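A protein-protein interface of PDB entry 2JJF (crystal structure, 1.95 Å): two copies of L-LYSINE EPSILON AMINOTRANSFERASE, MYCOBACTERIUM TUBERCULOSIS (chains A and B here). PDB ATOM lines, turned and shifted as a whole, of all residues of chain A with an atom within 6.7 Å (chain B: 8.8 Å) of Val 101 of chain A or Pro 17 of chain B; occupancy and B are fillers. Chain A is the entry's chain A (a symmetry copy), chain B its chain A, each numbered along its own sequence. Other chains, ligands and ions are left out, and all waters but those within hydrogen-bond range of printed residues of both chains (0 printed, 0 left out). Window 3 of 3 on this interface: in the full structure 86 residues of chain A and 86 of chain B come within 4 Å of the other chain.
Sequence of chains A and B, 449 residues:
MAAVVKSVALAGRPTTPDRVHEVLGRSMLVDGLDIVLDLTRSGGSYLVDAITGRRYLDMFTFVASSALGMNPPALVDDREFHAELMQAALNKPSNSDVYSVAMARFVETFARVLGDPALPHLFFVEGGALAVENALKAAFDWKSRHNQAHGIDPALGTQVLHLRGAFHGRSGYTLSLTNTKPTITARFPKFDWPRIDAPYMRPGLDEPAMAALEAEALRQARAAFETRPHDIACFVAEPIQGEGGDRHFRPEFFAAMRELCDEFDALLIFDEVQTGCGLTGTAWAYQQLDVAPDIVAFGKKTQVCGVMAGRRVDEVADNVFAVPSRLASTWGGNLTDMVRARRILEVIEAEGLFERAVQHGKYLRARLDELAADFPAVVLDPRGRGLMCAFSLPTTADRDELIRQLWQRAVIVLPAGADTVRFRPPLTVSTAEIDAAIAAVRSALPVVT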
ATOM      1  N   TYR A  99      -2.782  34.199  20.813  1.00  0.00           N
ATOM      2  CA  TYR A  99      -3.667  33.110  20.392  1.00  0.00           C
ATOM      3  C   TYR A  99      -3.688  31.965  21.383  1.00  0.00           C
ATOM      4  O   TYR A  99      -2.734  31.767  22.134  1.00  0.00           O
ATOM      5  CB  TYR A  99      -3.296  32.608  18.990  1.00  0.00           C
ATOM      6  CG  TYR A  99      -3.122  33.733  17.999  1.00  0.00           C
ATOM      7  CD1 TYR A  99      -4.106  34.715  17.843  1.00  0.00           C
ATOM      8  CD2 TYR A  99      -1.973  33.828  17.228  1.00  0.00           C
ATOM      9  CE1 TYR A  99      -3.941  35.763  16.950  1.00  0.00           C
ATOM     10  CE2 TYR A  99      -1.801  34.871  16.330  1.00  0.00           C
ATOM     11  CZ  TYR A  99      -2.785  35.830  16.196  1.00  0.00           C
ATOM     12  OH  TYR A  99      -2.608  36.853  15.292  1.00  0.00           O
ATOM     13  N   SER A 100      -4.795  31.226  21.385  1.00  0.00           N
ATOM     14  CA  SER A 100      -4.985  30.104  22.290  1.00  0.00           C
ATOM     15  C   SER A 100      -5.677  28.975  21.550  1.00  0.00           C
ATOM     16  O   SER A 100      -6.279  29.185  20.491  1.00  0.00           O
ATOM     17  CB  SER A 100      -5.834  30.510  23.499  1.00  0.00           C
ATOM     18  OG  SER A 100      -7.089  31.048  23.096  1.00  0.00           O
ATOM     19  N   VAL A 101      -5.602  27.779  22.124  1.00  0.00           N
ATOM     20  CA  VAL A 101      -6.355  26.645  21.607  1.00  0.00           C
ATOM     21  C   VAL A 101      -7.867  26.934  21.673  1.00  0.00           C
ATOM     22  O   VAL A 101      -8.602  26.623  20.738  1.00  0.00           O
ATOM     23  CB  VAL A 101      -6.011  25.350  22.370  1.00  0.00           C
ATOM     24  CG1 VAL A 101      -7.009  24.235  22.029  1.00  0.00           C
ATOM     25  CG2 VAL A 101      -4.568  24.908  22.045  1.00  0.00           C
ATOM     26  N   ALA A 102      -8.312  27.529  22.780  1.00  0.00           N
ATOM     27  CA  ALA A 102      -9.728  27.852  22.979  1.00  0.00           C
ATOM     28  C   ALA A 102     -10.257  28.716  21.834  1.00  0.00           C
ATOM     29  O   ALA A 102     -11.348  28.465  21.312  1.00  0.00           O
ATOM     30  CB  ALA A 102      -9.930  28.553  24.321  1.00  0.00           C
ATOM     31  N   MET A 103      -9.476  29.723  21.444  1.00  0.00           N
ATOM     32  CA  MET A 103      -9.825  30.583  20.315  1.00  0.00           C
ATOM     33  C   MET A 103      -9.847  29.831  18.975  1.00  0.00           C
ATOM     34  O   MET A 103     -10.796  29.976  18.196  1.00  0.00           O
ATOM     35  CB  MET A 103      -8.869  31.773  20.243  1.00  0.00           C
ATOM     36  CG  MET A 103      -9.121  32.712  19.067  1.00  0.00           C
ATOM     37  SD  MET A 103      -7.764  33.887  18.960  1.00  0.00           S
ATOM     38  CE  MET A 103      -8.229  34.788  17.477  1.00  0.00           C
ATOM     39  N   ALA A 104      -8.814  29.025  18.713  1.00  0.00           N
ATOM     40  CA  ALA A 104      -8.719  28.283  17.447  1.00  0.00           C
ATOM     41  C   ALA A 104      -9.864  27.286  17.282  1.00  0.00           C
ATOM     42  O   ALA A 104     -10.401  27.138  16.184  1.00  0.00           O
ATOM     43  CB  ALA A 104      -7.355  27.581  17.302  1.00  0.00           C
ATOM     44  N   ARG A 105     -10.234  26.608  18.366  1.00  0.00           N
ATOM     45  CA  ARG A 105     -11.389  25.705  18.358  1.00  0.00           C
ATOM     46  C   ARG A 105     -12.684  26.431  18.014  1.00  0.00           C
ATOM     47  O   ARG A 105     -13.521  25.898  17.271  1.00  0.00           O
ATOM     48  CB  ARG A 105     -11.546  24.985  19.701  1.00  0.00           C
ATOM     49  CG  ARG A 105     -10.470  23.944  19.979  1.00  0.00           C
ATOM     50  CD  ARG A 105     -10.678  23.274  21.333  1.00  0.00           C
ATOM     51  NE  ARG A 105     -11.873  22.423  21.361  1.00  0.00           N
ATOM     52  CZ  ARG A 105     -12.356  21.850  22.464  1.00  0.00           C
ATOM     53  NH1 ARG A 105     -11.754  22.029  23.638  1.00  0.00           N
ATOM     54  NH2 ARG A 105     -13.443  21.094  22.399  1.00  0.00           N
ATOM     55  N   PHE A 106     -12.865  27.636  18.560  1.00  0.00           N
ATOM     56  CA  PHE A 106     -14.049  28.431  18.229  1.00  0.00           C
ATOM     57  C   PHE A 106     -14.074  28.791  16.736  1.00  0.00           C
ATOM     58  O   PHE A 106     -15.095  28.622  16.062  1.00  0.00           O
ATOM     59  CB  PHE A 106     -14.148  29.704  19.082  1.00  0.00           C
ATOM     60  CG  PHE A 106     -14.997  30.768  18.453  1.00  0.00           C
ATOM     61  CD1 PHE A 106     -16.389  30.651  18.438  1.00  0.00           C
ATOM     62  CD2 PHE A 106     -14.408  31.864  17.834  1.00  0.00           C
ATOM     63  CE1 PHE A 106     -17.181  31.622  17.826  1.00  0.00           C
ATOM     64  CE2 PHE A 106     -15.195  32.842  17.220  1.00  0.00           C
ATOM     65  CZ  PHE A 106     -16.580  32.717  17.214  1.00  0.00           C
ATOM     66  N   GLU A 108     -12.543  27.420  14.112  1.00  0.00           N
ATOM     67  CA  GLU A 108     -12.795  26.273  13.234  1.00  0.00           C
ATOM     68  C   GLU A 108     -14.246  25.782  13.281  1.00  0.00           C
ATOM     69  O   GLU A 108     -14.790  25.399  12.246  1.00  0.00           O
ATOM     70  CB  GLU A 108     -11.797  25.124  13.449  1.00  0.00           C
ATOM     71  CG  GLU A 108     -11.823  24.487  14.817  1.00  0.00           C
ATOM     72  CD  GLU A 108     -10.927  23.251  14.923  1.00  0.00           C
ATOM     73  OE1 GLU A 108     -10.283  22.853  13.913  1.00  0.00           O
ATOM     74  OE2 GLU A 108     -10.890  22.667  16.032  1.00  0.00           O
ATOM     75  N   LEU A 335     -12.995  36.207  24.862  1.00  0.00           N
ATOM     76  CA  LEU A 335     -12.667  34.764  24.823  1.00  0.00           C
ATOM     77  C   LEU A 335     -13.743  33.885  25.485  1.00  0.00           C
ATOM     78  O   LEU A 335     -14.033  32.789  25.002  1.00  0.00           O
ATOM     79  CB  LEU A 335     -11.295  34.476  25.438  1.00  0.00           C
ATOM     80  CG  LEU A 335     -10.766  33.037  25.313  1.00  0.00           C
ATOM     81  CD1 LEU A 335     -10.558  32.628  23.842  1.00  0.00           C
ATOM     82  CD2 LEU A 335      -9.485  32.869  26.108  1.00  0.00           C
ATOM     83  N   THR B  15      -7.669  20.046  17.989  1.00  0.00           N
ATOM     84  CA  THR B  15      -6.620  21.021  17.565  1.00  0.00           C
ATOM     85  C   THR B  15      -5.634  21.257  18.704  1.00  0.00           C
ATOM     86  O   THR B  15      -6.014  21.559  19.839  1.00  0.00           O
ATOM     87  CB  THR B  15      -7.215  22.348  16.980  1.00  0.00           C
ATOM     88  OG1 THR B  15      -6.252  23.412  17.066  1.00  0.00           O
ATOM     89  CG2 THR B  15      -8.449  22.754  17.725  1.00  0.00           C
ATOM     90  N   THR B  16      -4.364  21.090  18.373  1.00  0.00           N
ATOM     91  CA  THR B  16      -3.276  21.065  19.337  1.00  0.00           C
ATOM     92  C   THR B  16      -2.542  22.416  19.292  1.00  0.00           C
ATOM     93  O   THR B  16      -2.632  23.117  18.288  1.00  0.00           O
ATOM     94  CB  THR B  16      -2.344  19.859  19.013  1.00  0.00           C
ATOM     95  OG1 THR B  16      -1.032  20.085  19.534  1.00  0.00           O
ATOM     96  CG2 THR B  16      -2.232  19.653  17.513  1.00  0.00           C
ATOM     97  N   PRO B  17      -1.847  22.806  20.384  1.00  0.00           N
ATOM     98  CA  PRO B  17      -1.110  24.080  20.380  1.00  0.00           C
ATOM     99  C   PRO B  17      -0.287  24.350  19.111  1.00  0.00           C
ATOM    100  O   PRO B  17      -0.304  25.467  18.592  1.00  0.00           O
ATOM    101  CB  PRO B  17      -0.192  23.954  21.600  1.00  0.00           C
ATOM    102  CG  PRO B  17      -0.954  23.111  22.538  1.00  0.00           C
ATOM    103  CD  PRO B  17      -1.738  22.129  21.693  1.00  0.00           C
ATOM    104  N   ASP B  18       0.415  23.335  18.613  1.00  0.00           N
ATOM    105  CA  ASP B  18       1.265  23.508  17.431  1.00  0.00           C
ATOM    106  C   ASP B  18       0.485  23.689  16.111  1.00  0.00           C
ATOM    107  O   ASP B  18       1.074  24.025  15.086  1.00  0.00           O
ATOM    108  CB  ASP B  18       2.275  22.356  17.323  1.00  0.00           C
ATOM    109  CG  ASP B  18       1.619  21.043  16.963  1.00  0.00           C
ATOM    110  OD1 ASP B  18       0.680  20.618  17.667  1.00  0.00           O
ATOM    111  OD2 ASP B  18       2.039  20.435  15.961  1.00  0.00           O
ATOM    112  N   ARG B  19      -0.830  23.482  16.146  1.00  0.00           N
ATOM    113  CA  ARG B  19      -1.689  23.695  14.971  1.00  0.00           C
ATOM    114  C   ARG B  19      -2.562  24.965  15.037  1.00  0.00           C
ATOM    115  O   ARG B  19      -3.330  25.244  14.105  1.00  0.00           O
ATOM    116  CB  ARG B  19      -2.577  22.471  14.721  1.00  0.00           C
ATOM    117  CG  ARG B  19      -1.827  21.234  14.210  1.00  0.00           C
ATOM    118  CD  ARG B  19      -2.666  20.401  13.229  1.00  0.00           C
ATOM    119  NE  ARG B  19      -4.086  20.357  13.590  1.00  0.00           N
ATOM    120  CZ  ARG B  19      -5.077  20.801  12.817  1.00  0.00           C
ATOM    121  NH1 ARG B  19      -4.820  21.313  11.614  1.00  0.00           N
ATOM    122  NH2 ARG B  19      -6.336  20.725  13.244  1.00  0.00           N
ATOM    123  N   VAL B  20      -2.444  25.727  16.127  1.00  0.00           N
ATOM    124  CA  VAL B  20      -3.258  26.928  16.337  1.00  0.00           C
ATOM    125  C   VAL B  20      -3.073  27.970  15.227  1.00  0.00           C
ATOM    126  O   VAL B  20      -4.053  28.438  14.658  1.00  0.00           O
ATOM    127  CB  VAL B  20      -3.010  27.543  17.748  1.00  0.00           C
ATOM    128  CG1 VAL B  20      -3.484  29.001  17.829  1.00  0.00           C
ATOM    129  CG2 VAL B  20      -3.689  26.694  18.814  1.00  0.00           C
ATOM    130  N   HIS B  21      -1.824  28.317  14.919  1.00  0.00           N
ATOM    131  CA  HIS B  21      -1.525  29.329  13.906  1.00  0.00           C
ATOM    132  C   HIS B  21      -1.993  28.918  12.505  1.00  0.00           C
ATOM    133  O   HIS B  21      -2.462  29.763  11.732  1.00  0.00           O
ATOM    134  CB  HIS B  21      -0.030  29.681  13.904  1.00  0.00           C
ATOM    135  CG  HIS B  21       0.414  30.433  15.121  1.00  0.00           C
ATOM    136  ND1 HIS B  21       0.718  31.776  15.097  1.00  0.00           N
ATOM    137  CD2 HIS B  21       0.597  30.029  16.402  1.00  0.00           C
ATOM    138  CE1 HIS B  21       1.074  32.167  16.307  1.00  0.00           C
ATOM    139  NE2 HIS B  21       1.006  31.127  17.119  1.00  0.00           N
ATOM    140  N   GLU B  22      -1.870  27.627  12.202  1.00  0.00           N
ATOM    141  CA  GLU B  22      -2.355  27.050  10.951  1.00  0.00           C
ATOM    142  C   GLU B  22      -3.879  27.166  10.811  1.00  0.00           C
ATOM    143  O   GLU B  22      -4.371  27.620   9.779  1.00  0.00           O
ATOM    144  CB  GLU B  22      -1.926  25.583  10.851  1.00  0.00           C
ATOM    145  CG  GLU B  22      -2.524  24.833   9.663  1.00  0.00           C
ATOM    146  CD  GLU B  22      -2.321  23.324   9.745  1.00  0.00           C
ATOM    147  OE1 GLU B  22      -1.401  22.868  10.467  1.00  0.00           O
ATOM    148  OE2 GLU B  22      -3.088  22.593   9.079  1.00  0.00           O
ATOM    149  N   VAL B  23      -4.610  26.769  11.854  1.00  0.00           N
ATOM    150  CA  VAL B  23      -6.078  26.825  11.865  1.00  0.00           C
ATOM    151  C   VAL B  23      -6.587  28.266  11.725  1.00  0.00           C
ATOM    152  O   VAL B  23      -7.447  28.545  10.885  1.00  0.00           O
ATOM    153  CB  VAL B  23      -6.680  26.127  13.119  1.00  0.00           C
ATOM    154  CG1 VAL B  23      -8.184  26.324  13.184  1.00  0.00           C
ATOM    155  CG2 VAL B  23      -6.350  24.629  13.120  1.00  0.00           C
ATOM    156  N   LEU B  24      -6.042  29.177  12.526  1.00  0.00           N
ATOM    157  CA  LEU B  24      -6.445  30.581  12.467  1.00  0.00           C
ATOM    158  C   LEU B  24      -6.087  31.211  11.126  1.00  0.00           C
ATOM    159  O   LEU B  24      -6.848  32.028  10.596  1.00  0.00           O
ATOM    160  CB  LEU B  24      -5.812  31.391  13.611  1.00  0.00           C
ATOM    161  CG  LEU B  24      -6.217  31.043  15.044  1.00  0.00           C
ATOM    162  CD1 LEU B  24      -5.374  31.831  16.033  1.00  0.00           C
ATOM    163  CD2 LEU B  24      -7.696  31.296  15.276  1.00  0.00           C
ATOM    164  N   ASP B  34       4.336  34.962  18.529  1.00  0.00           N
ATOM    165  CA  ASP B  34       4.687  33.611  18.081  1.00  0.00           C
ATOM    166  C   ASP B  34       4.226  32.472  18.988  1.00  0.00           C
ATOM    167  O   ASP B  34       4.197  31.303  18.570  1.00  0.00           O
ATOM    168  CB  ASP B  34       6.195  33.500  17.868  1.00  0.00           C
ATOM    169  CG  ASP B  34       6.588  33.715  16.435  1.00  0.00           C
ATOM    170  OD1 ASP B  34       5.758  34.237  15.650  1.00  0.00           O
ATOM    171  OD2 ASP B  34       7.737  33.355  16.089  1.00  0.00           O
ATOM    172  N   ILE B  35       3.863  32.810  20.216  1.00  0.00           N
ATOM    173  CA  ILE B  35       3.510  31.804  21.209  1.00  0.00           C
ATOM    174  C   ILE B  35       2.042  31.387  21.114  1.00  0.00           C
ATOM    175  O   ILE B  35       1.251  32.002  20.390  1.00  0.00           O
ATOM    176  CB  ILE B  35       3.829  32.304  22.639  1.00  0.00           C
ATOM    177  CG1 ILE B  35       2.990  33.542  22.980  1.00  0.00           C
ATOM    178  CG2 ILE B  35       5.339  32.592  22.776  1.00  0.00           C
ATOM    179  CD1 ILE B  35       2.837  33.786  24.466  1.00  0.00           C
ATOM    180  N   VAL B  36       1.704  30.328  21.839  1.00  0.00           N
ATOM    181  CA  VAL B  36       0.320  29.963  22.083  1.00  0.00           C
ATOM    182  C   VAL B  36       0.126  30.033  23.592  1.00  0.00           C
ATOM    183  O   VAL B  36       0.855  29.380  24.348  1.00  0.00           O
ATOM    184  CB  VAL B  36      -0.014  28.554  21.523  1.00  0.00           C
ATOM    185  CG1 VAL B  36      -1.428  28.105  21.938  1.00  0.00           C
ATOM    186  CG2 VAL B  36       0.122  28.549  20.005  1.00  0.00           C
ATOM    187  N   LEU B  37      -0.839  30.840  24.030  1.00  0.00           N
ATOM    188  CA  LEU B  37      -1.059  31.082  25.456  1.00  0.00           C
ATOM    189  C   LEU B  37      -1.564  29.832  26.168  1.00  0.00           C
ATOM    190  O   LEU B  37      -2.607  29.289  25.807  1.00  0.00           O
ATOM    191  CB  LEU B  37      -2.097  32.200  25.656  1.00  0.00           C
ATOM    192  CG  LEU B  37      -1.978  33.245  26.781  1.00  0.00           C
ATOM    193  CD1 LEU B  37      -3.358  33.693  27.275  1.00  0.00           C
ATOM    194  CD2 LEU B  37      -1.074  32.831  27.931  1.00  0.00           C
ATOM    195  N   ASP B  38      -0.833  29.395  27.190  1.00  0.00           N
ATOM    196  CA  ASP B  38      -1.313  28.362  28.092  1.00  0.00           C
ATOM    197  C   ASP B  38      -2.173  29.033  29.162  1.00  0.00           C
ATOM    198  O   ASP B  38      -1.644  29.714  30.042  1.00  0.00           O
ATOM    199  CB  ASP B  38      -0.131  27.629  28.735  1.00  0.00           C
ATOM    200  CG  ASP B  38      -0.557  26.409  29.537  1.00  0.00           C
ATOM    201  OD1 ASP B  38      -1.572  26.461  30.265  1.00  0.00           O
ATOM    202  OD2 ASP B  38       0.142  25.383  29.444  1.00  0.00           O
ATOM    203  N   LEU B  39      -3.490  28.829  29.089  1.00  0.00           N
ATOM    204  CA  LEU B  39      -4.448  29.522  29.958  1.00  0.00           C
ATOM    205  C   LEU B  39      -4.366  29.085  31.406  1.00  0.00           C
ATOM    206  O   LEU B  39      -4.768  29.825  32.300  1.00  0.00           O
ATOM    207  CB  LEU B  39      -5.892  29.330  29.456  1.00  0.00           C
ATOM    208  CG  LEU B  39      -6.235  29.883  28.068  1.00  0.00           C
ATOM    209  CD1 LEU B  39      -7.738  29.684  27.764  1.00  0.00           C
ATOM    210  CD2 LEU B  39      -5.878  31.344  27.985  1.00  0.00           C
ATOM    211  N   ARG B  41      -1.372  27.381  32.936  1.00  0.00           N
ATOM    212  CA  ARG B  41      -0.054  27.438  33.570  1.00  0.00           C
ATOM    213  C   ARG B  41       0.532  28.842  33.694  1.00  0.00           C
ATOM    214  O   ARG B  41       1.445  29.060  34.501  1.00  0.00           O
ATOM    215  CB  ARG B  41       0.914  26.463  32.905  1.00  0.00           C
ATOM    216  CG  ARG B  41       0.603  25.028  33.311  1.00  0.00           C
ATOM    217  CD  ARG B  41       1.522  24.038  32.631  1.00  0.00           C
ATOM    218  NE  ARG B  41       0.903  23.519  31.421  1.00  0.00           N
ATOM    219  CZ  ARG B  41       0.257  22.361  31.337  1.00  0.00           C
ATOM    220  NH1 ARG B  41       0.152  21.565  32.392  1.00  0.00           N
ATOM    221  NH2 ARG B  41      -0.278  21.995  30.183  1.00  0.00           N
ATOM    222  N   ASP B  49       4.161  29.763  27.136  1.00  0.00           N
ATOM    223  CA  ASP B  49       3.960  29.286  25.778  1.00  0.00           C
ATOM    224  C   ASP B  49       3.591  27.809  25.856  1.00  0.00           C
ATOM    225  O   ASP B  49       4.355  26.998  26.389  1.00  0.00           O
ATOM    226  CB  ASP B  49       5.232  29.500  24.937  1.00  0.00           C
ATOM    227  CG  ASP B  49       5.135  28.875  23.535  1.00  0.00           C
ATOM    228  OD1 ASP B  49       4.020  28.760  22.980  1.00  0.00           O
ATOM    229  OD2 ASP B  49       6.189  28.492  22.988  1.00  0.00           O
ATOM    230  N   ALA B  50       2.413  27.461  25.343  1.00  0.00           N
ATOM    231  CA  ALA B  50       1.936  26.079  25.405  1.00  0.00           C
ATOM    232  C   ALA B  50       2.753  25.130  24.521  1.00  0.00           C
ATOM    233  O   ALA B  50       2.730  23.922  24.738  1.00  0.00           O
ATOM    234  CB  ALA B  50       0.458  25.998  25.049  1.00  0.00           C
ATOM    235  N   ILE B  51       3.462  25.670  23.534  1.00  0.00           N
ATOM    236  CA  ILE B  51       4.266  24.855  22.616  1.00  0.00           C
ATOM    237  C   ILE B  51       5.566  24.378  23.297  1.00  0.00           C
ATOM    238  O   ILE B  51       5.842  23.177  23.332  1.00  0.00           O
ATOM    239  CB  ILE B  51       4.568  25.605  21.290  1.00  0.00           C
ATOM    240  CG1 ILE B  51       3.270  25.849  20.501  1.00  0.00           C
ATOM    241  CG2 ILE B  51       5.574  24.826  20.420  1.00  0.00           C
ATOM    242  CD1 ILE B  51       3.394  26.947  19.466  1.00  0.00           C
ATOM    243  N   THR B  52       6.337  25.310  23.857  1.00  0.00           N
ATOM    244  CA  THR B  52       7.654  24.986  24.449  1.00  0.00           C
ATOM    245  C   THR B  52       7.649  24.866  25.973  1.00  0.00           C
ATOM    246  O   THR B  52       8.507  24.194  26.551  1.00  0.00           O
ATOM    247  CB  THR B  52       8.720  26.034  24.073  1.00  0.00           C
ATOM    248  OG1 THR B  52       8.294  27.333  24.514  1.00  0.00           O
ATOM    249  CG2 THR B  52       8.950  26.057  22.568  1.00  0.00           C
ATOM    250  N   GLY B  53       6.692  25.518  26.627  1.00  0.00           N
ATOM    251  CA  GLY B  53       6.708  25.615  28.085  1.00  0.00           C
ATOM    252  C   GLY B  53       7.605  26.746  28.585  1.00  0.00           C
ATOM    253  O   GLY B  53       7.793  26.898  29.785  1.00  0.00           O
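The backbone carbonyl oxygen of Tyr 99 of chain A is in hydrogen-bond range of the backbone NH of Leu 37 of chain B, at 2.8 Å.
CB of Tyr 99 of chain A touches CG1 of Val 20 of chain B, 3.8 Å away.
CD2 of Tyr 99 of chain A touches CE1 of His 21 of chain B, at 3.6 Å.
Tyr 99 of chain A touches Leu 24 of chain B.
Tyr 99 of chain A touches Val 36 of chain B.
CG1 of Val 20 of chain B touches O of Ser 100 of chain A, 3.9 Å away.
Val 101 of chain A touches Thr 15 of chain B (CG1 to O, 3.6 Å).
N of Pro 17 of chain B touches CG2 of Val 101 of chain A, 3.8 Å away.
CG2 of Val 101 of chain A touches CG2 of Val 20 of chain B, 3.8 Å away.
Ala 104 of chain A touches Val 23 of chain B.
Leu 24 of chain B touches Ala 104 of chain A.
Hydrophobic or aromatic side chains of chain A within 4 Å of the printed part of chain B: Tyr 99, Val 101 and Leu 335.
Hydrophobic or aromatic side chains of chain B within 4 Å of the printed part of chain A: Pro 17, Val 20, His 21, Val 23, Leu 24, Val 36, Leu 37 and Leu 39.
Among the printed residues, no Asp or Glu carboxylate lies within 4 Å of a Lys or Arg side-chain nitrogen of the other chain.
Val 101 of chain A touches just these residues of chain B: Thr 15, Pro 17 and Val 20.
Of chain A, only Val 101 comes within 4 Å of Pro 17 of chain B.
Of chain B, only Val 20 (3.9 Å) comes within 4 Å of Ser 100 of chain A.
Printed residues of chain B within 4 Å of Tyr 99 of chain A: Val 20 (3.8 Å), His 21 (3.6 Å), Leu 24 (3.5 Å), Val 36 (3.5 Å) and Leu 37 (2.8 Å).
Of the printed residues of chain A, Leu 37 of chain B touches Tyr 99 (2.8 Å).
OG of Ser 100 of chain A sits at hydrogen-bond distance from N of Met 103 of chain A (3.2 Å).
A ring nitrogen (NE2) of His 21 of chain B lies within hydrogen-bond range of the backbone carbonyl oxygen (O) of Ile 35 of chain B (3.4 Å).
The backbone carbonyl oxygen (O) of Val 36 of chain B lies within hydrogen-bond range of the backbone NH (N) of Ala 50 of chain B, 2.7 Å away.
N of Val 36 of chain B sits at hydrogen-bond distance from OD1 of Asp 49 of chain B (3.0 Å).
No position is printed for both chains.
Of the 15 pairs that touch across the chains among the printed residues, none has its exchanged pair printed and touching as well.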
